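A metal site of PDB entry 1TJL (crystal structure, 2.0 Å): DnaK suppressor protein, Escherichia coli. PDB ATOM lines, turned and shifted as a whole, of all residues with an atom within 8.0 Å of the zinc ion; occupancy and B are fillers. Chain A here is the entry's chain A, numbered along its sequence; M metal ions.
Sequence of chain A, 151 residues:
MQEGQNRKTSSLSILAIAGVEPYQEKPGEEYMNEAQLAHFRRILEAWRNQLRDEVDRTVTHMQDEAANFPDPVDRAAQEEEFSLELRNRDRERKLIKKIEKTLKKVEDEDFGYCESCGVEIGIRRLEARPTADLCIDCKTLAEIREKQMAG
The side-chain sulfur (SG) of Cys 114 lies close to the backbone NH (N) of Ser 116, at 3.2 Å. The backbone NH (N) of Cys 114 lies within hydrogen-bond range of the backbone carbonyl oxygen (O) of Val 119 (2.5 Å). The backbone NH of Val 119 sits close to the side-chain sulfur of Cys 117 (3.8 Å). SG of Cys 135 sits close to N of Asp 137 (3.8 Å).
The side-chain sulfur (SG) of Cys 138 is bound to the zinc ion, at 2.3 Å. SG of Cys 114 is bound to the zinc ion (2.3 Å). SG of Cys 117 binds the zinc ion (2.3 Å). SG of Cys 135 binds the zinc ion, 2.4 Å away. The zinc ion has four donor atoms within binding distance.
Four residues have an atom within 4 Å of the zinc ion: Cys 114, Cys 117, Cys 135 and Cys 138.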
ATOM      1  N   TYR A 113     -28.788  22.706  -0.337  1.00  0.00           N
ATOM      2  CA  TYR A 113     -27.502  22.825  -1.024  1.00  0.00           C
ATOM      3  C   TYR A 113     -26.458  21.823  -0.540  1.00  0.00           C
ATOM      4  O   TYR A 113     -26.533  21.315   0.571  1.00  0.00           O
ATOM      5  CB  TYR A 113     -26.946  24.252  -0.849  1.00  0.00           C
ATOM      6  CG  TYR A 113     -27.873  25.312  -1.353  1.00  0.00           C
ATOM      7  CD1 TYR A 113     -28.931  25.768  -0.564  1.00  0.00           C
ATOM      8  CD2 TYR A 113     -27.707  25.839  -2.629  1.00  0.00           C
ATOM      9  CE1 TYR A 113     -29.800  26.723  -1.038  1.00  0.00           C
ATOM     10  CE2 TYR A 113     -28.573  26.796  -3.117  1.00  0.00           C
ATOM     11  CZ  TYR A 113     -29.628  27.232  -2.328  1.00  0.00           C
ATOM     12  OH  TYR A 113     -30.499  28.179  -2.847  1.00  0.00           O
ATOM     13  N   CYS A 114     -25.480  21.561  -1.396  1.00  0.00           N
ATOM     14  CA  CYS A 114     -24.420  20.628  -1.073  1.00  0.00           C
ATOM     15  C   CYS A 114     -23.579  21.200   0.052  1.00  0.00           C
ATOM     16  O   CYS A 114     -23.213  22.386   0.021  1.00  0.00           O
ATOM     17  CB  CYS A 114     -23.528  20.357  -2.292  1.00  0.00           C
ATOM     18  SG  CYS A 114     -21.994  19.488  -1.866  1.00  0.00           S
ATOM     19  N   GLU A 115     -23.251  20.380   1.047  1.00  0.00           N
ATOM     20  CA  GLU A 115     -22.461  20.865   2.157  1.00  0.00           C
ATOM     21  C   GLU A 115     -20.972  21.019   1.826  1.00  0.00           C
ATOM     22  O   GLU A 115     -20.281  21.769   2.502  1.00  0.00           O
ATOM     23  CB  GLU A 115     -22.640  19.944   3.376  1.00  0.00           C
ATOM     24  CG  GLU A 115     -24.099  19.818   3.872  1.00  0.00           C
ATOM     25  CD  GLU A 115     -24.235  19.179   5.273  1.00  0.00           C
ATOM     26  OE1 GLU A 115     -23.346  18.381   5.662  1.00  0.00           O
ATOM     27  OE2 GLU A 115     -25.243  19.453   5.973  1.00  0.00           O
ATOM     28  N   SER A 116     -20.477  20.299   0.819  1.00  0.00           N
ATOM     29  CA  SER A 116     -19.071  20.393   0.445  1.00  0.00           C
ATOM     30  C   SER A 116     -18.825  21.594  -0.445  1.00  0.00           C
ATOM     31  O   SER A 116     -17.997  22.449  -0.157  1.00  0.00           O
ATOM     32  CB  SER A 116     -18.630  19.119  -0.282  1.00  0.00           C
ATOM     33  OG  SER A 116     -18.200  18.125   0.617  1.00  0.00           O
ATOM     34  N   CYS A 117     -19.545  21.655  -1.559  1.00  0.00           N
ATOM     35  CA  CYS A 117     -19.444  22.786  -2.459  1.00  0.00           C
ATOM     36  C   CYS A 117     -20.802  23.466  -2.312  1.00  0.00           C
ATOM     37  O   CYS A 117     -21.780  22.808  -1.978  1.00  0.00           O
ATOM     38  CB  CYS A 117     -19.180  22.281  -3.883  1.00  0.00           C
ATOM     39  SG  CYS A 117     -20.554  21.461  -4.729  1.00  0.00           S
ATOM     40  N   GLY A 118     -20.893  24.756  -2.553  1.00  0.00           N
ATOM     41  CA  GLY A 118     -22.178  25.414  -2.343  1.00  0.00           C
ATOM     42  C   GLY A 118     -23.348  25.018  -3.238  1.00  0.00           C
ATOM     43  O   GLY A 118     -24.479  25.434  -2.989  1.00  0.00           O
ATOM     44  N   VAL A 119     -23.068  24.218  -4.261  1.00  0.00           N
ATOM     45  CA  VAL A 119     -24.043  23.763  -5.238  1.00  0.00           C
ATOM     46  C   VAL A 119     -25.418  23.374  -4.686  1.00  0.00           C
ATOM     47  O   VAL A 119     -25.530  22.841  -3.588  1.00  0.00           O
ATOM     48  CB  VAL A 119     -23.471  22.561  -6.039  1.00  0.00           C
ATOM     49  CG1 VAL A 119     -24.523  21.918  -6.898  1.00  0.00           C
ATOM     50  CG2 VAL A 119     -22.321  23.020  -6.893  1.00  0.00           C
ATOM     51  N   GLU A 120     -26.452  23.630  -5.476  1.00  0.00           N
ATOM     52  CA  GLU A 120     -27.796  23.272  -5.068  1.00  0.00           C
ATOM     53  C   GLU A 120     -27.996  21.810  -5.402  1.00  0.00           C
ATOM     54  O   GLU A 120     -27.543  21.348  -6.430  1.00  0.00           O
ATOM     55  CB  GLU A 120     -28.829  24.094  -5.835  1.00  0.00           C
ATOM     56  CG  GLU A 120     -28.386  25.505  -6.202  1.00  0.00           C
ATOM     57  CD  GLU A 120     -29.455  26.252  -6.993  1.00  0.00           C
ATOM     58  OE1 GLU A 120     -29.962  25.682  -7.993  1.00  0.00           O
ATOM     59  OE2 GLU A 120     -29.783  27.404  -6.620  1.00  0.00           O
ATOM     60  N   ILE A 121     -28.657  21.076  -4.520  1.00  0.00           N
ATOM     61  CA  ILE A 121     -28.950  19.667  -4.736  1.00  0.00           C
ATOM     62  C   ILE A 121     -30.291  19.646  -5.473  1.00  0.00           C
ATOM     63  O   ILE A 121     -31.185  20.437  -5.186  1.00  0.00           O
ATOM     64  CB  ILE A 121     -29.077  18.921  -3.394  1.00  0.00           C
ATOM     65  CG1 ILE A 121     -27.704  18.919  -2.708  1.00  0.00           C
ATOM     66  CG2 ILE A 121     -29.619  17.508  -3.622  1.00  0.00           C
ATOM     67  CD1 ILE A 121     -27.699  18.301  -1.340  1.00  0.00           C
ATOM     68  N   ARG A 125     -34.058  15.393  -6.629  1.00  0.00           N
ATOM     69  CA  ARG A 125     -33.143  14.544  -5.875  1.00  0.00           C
ATOM     70  C   ARG A 125     -33.472  14.612  -4.386  1.00  0.00           C
ATOM     71  O   ARG A 125     -33.373  13.608  -3.670  1.00  0.00           O
ATOM     72  CB  ARG A 125     -31.688  14.941  -6.072  1.00  0.00           C
ATOM     73  CG  ARG A 125     -30.806  14.033  -5.207  1.00  0.00           C
ATOM     74  CD  ARG A 125     -29.360  14.429  -5.148  1.00  0.00           C
ATOM     75  NE  ARG A 125     -28.696  13.675  -4.089  1.00  0.00           N
ATOM     76  CZ  ARG A 125     -27.446  13.888  -3.687  1.00  0.00           C
ATOM     77  NH1 ARG A 125     -26.738  14.850  -4.273  1.00  0.00           N
ATOM     78  NH2 ARG A 125     -26.920  13.167  -2.703  1.00  0.00           N
ATOM     79  N   ASP A 133     -27.021  15.457   2.064  1.00  0.00           N
ATOM     80  CA  ASP A 133     -26.043  16.449   2.516  1.00  0.00           C
ATOM     81  C   ASP A 133     -25.106  16.898   1.402  1.00  0.00           C
ATOM     82  O   ASP A 133     -24.558  18.005   1.446  1.00  0.00           O
ATOM     83  CB  ASP A 133     -25.146  15.877   3.633  1.00  0.00           C
ATOM     84  CG  ASP A 133     -25.920  15.198   4.745  1.00  0.00           C
ATOM     85  OD1 ASP A 133     -26.671  14.222   4.477  1.00  0.00           O
ATOM     86  OD2 ASP A 133     -25.759  15.612   5.907  1.00  0.00           O
ATOM     87  N   LEU A 134     -24.886  16.027   0.416  1.00  0.00           N
ATOM     88  CA  LEU A 134     -23.965  16.351  -0.661  1.00  0.00           C
ATOM     89  C   LEU A 134     -24.548  16.270  -2.049  1.00  0.00           C
ATOM     90  O   LEU A 134     -25.548  15.581  -2.285  1.00  0.00           O
ATOM     91  CB  LEU A 134     -22.770  15.417  -0.594  1.00  0.00           C
ATOM     92  CG  LEU A 134     -22.049  15.630   0.749  1.00  0.00           C
ATOM     93  CD1 LEU A 134     -20.888  14.668   0.893  1.00  0.00           C
ATOM     94  CD2 LEU A 134     -21.561  17.071   0.846  1.00  0.00           C
ATOM     95  N   CYS A 135     -23.944  17.048  -2.959  1.00  0.00           N
ATOM     96  CA  CYS A 135     -24.354  16.961  -4.328  1.00  0.00           C
ATOM     97  C   CYS A 135     -23.783  15.558  -4.631  1.00  0.00           C
ATOM     98  O   CYS A 135     -22.928  15.055  -3.881  1.00  0.00           O
ATOM     99  CB  CYS A 135     -23.709  18.067  -5.193  1.00  0.00           C
ATOM    100  SG  CYS A 135     -21.927  17.966  -5.424  1.00  0.00           S
ATOM    101  N   ILE A 136     -24.248  14.926  -5.697  1.00  0.00           N
ATOM    102  CA  ILE A 136     -23.782  13.580  -6.024  1.00  0.00           C
ATOM    103  C   ILE A 136     -22.267  13.457  -6.142  1.00  0.00           C
ATOM    104  O   ILE A 136     -21.697  12.479  -5.673  1.00  0.00           O
ATOM    105  CB  ILE A 136     -24.428  13.052  -7.326  1.00  0.00           C
ATOM    106  CG1 ILE A 136     -25.940  12.890  -7.142  1.00  0.00           C
ATOM    107  CG2 ILE A 136     -23.852  11.714  -7.703  1.00  0.00           C
ATOM    108  CD1 ILE A 136     -26.669  14.208  -7.046  1.00  0.00           C
ATOM    109  N   ASP A 137     -21.624  14.451  -6.750  1.00  0.00           N
ATOM    110  CA  ASP A 137     -20.179  14.421  -6.924  1.00  0.00           C
ATOM    111  C   ASP A 137     -19.432  14.416  -5.599  1.00  0.00           C
ATOM    112  O   ASP A 137     -18.578  13.569  -5.372  1.00  0.00           O
ATOM    113  CB  ASP A 137     -19.689  15.604  -7.754  1.00  0.00           C
ATOM    114  CG  ASP A 137     -20.513  15.848  -9.001  1.00  0.00           C
ATOM    115  OD1 ASP A 137     -21.752  16.010  -8.876  1.00  0.00           O
ATOM    116  OD2 ASP A 137     -19.912  15.905 -10.108  1.00  0.00           O
ATOM    117  N   CYS A 138     -19.732  15.372  -4.732  1.00  0.00           N
ATOM    118  CA  CYS A 138     -19.047  15.441  -3.455  1.00  0.00           C
ATOM    119  C   CYS A 138     -19.394  14.237  -2.624  1.00  0.00           C
ATOM    120  O   CYS A 138     -18.560  13.722  -1.897  1.00  0.00           O
ATOM    121  CB  CYS A 138     -19.412  16.703  -2.678  1.00  0.00           C
ATOM    122  SG  CYS A 138     -18.784  18.245  -3.381  1.00  0.00           S
ATOM    123  N   LYS A 139     -20.647  13.810  -2.719  1.00  0.00           N
ATOM    124  CA  LYS A 139     -21.089  12.646  -1.963  1.00  0.00           C
ATOM    125  C   LYS A 139     -20.278  11.433  -2.359  1.00  0.00           C
ATOM    126  O   LYS A 139     -19.782  10.693  -1.517  1.00  0.00           O
ATOM    127  CB  LYS A 139     -22.566  12.345  -2.237  1.00  0.00           C
ATOM    128  CG  LYS A 139     -23.030  11.031  -1.588  1.00  0.00           C
ATOM    129  CD  LYS A 139     -24.371  10.527  -2.134  1.00  0.00           C
ATOM    130  CE  LYS A 139     -24.805   9.235  -1.423  1.00  0.00           C
ATOM    131  NZ  LYS A 139     -25.859   8.486  -2.151  1.00  0.00           N
ATOM    132  N   ARG A 145     -12.988   8.518  -0.988  1.00  0.00           N
ATOM    133  CA  ARG A 145     -11.941   8.873  -0.035  1.00  0.00           C
ATOM    134  C   ARG A 145     -12.024   7.907   1.133  1.00  0.00           C
ATOM    135  O   ARG A 145     -11.009   7.426   1.634  1.00  0.00           O
ATOM    136  CB  ARG A 145     -12.123  10.282   0.510  1.00  0.00           C
ATOM    137  CG  ARG A 145     -12.327  11.364  -0.516  1.00  0.00           C
ATOM    138  CD  ARG A 145     -12.578  12.718   0.138  1.00  0.00           C
ATOM    139  NE  ARG A 145     -13.307  13.619  -0.765  1.00  0.00           N
ATOM    140  CZ  ARG A 145     -13.695  14.856  -0.454  1.00  0.00           C
ATOM    141  NH1 ARG A 145     -13.424  15.354   0.747  1.00  0.00           N
ATOM    142  NH2 ARG A 145     -14.371  15.582  -1.333  1.00  0.00           N
HETATM  143 ZN    ZN M   1     -20.757  19.305  -3.836  1.00  0.00          ZN
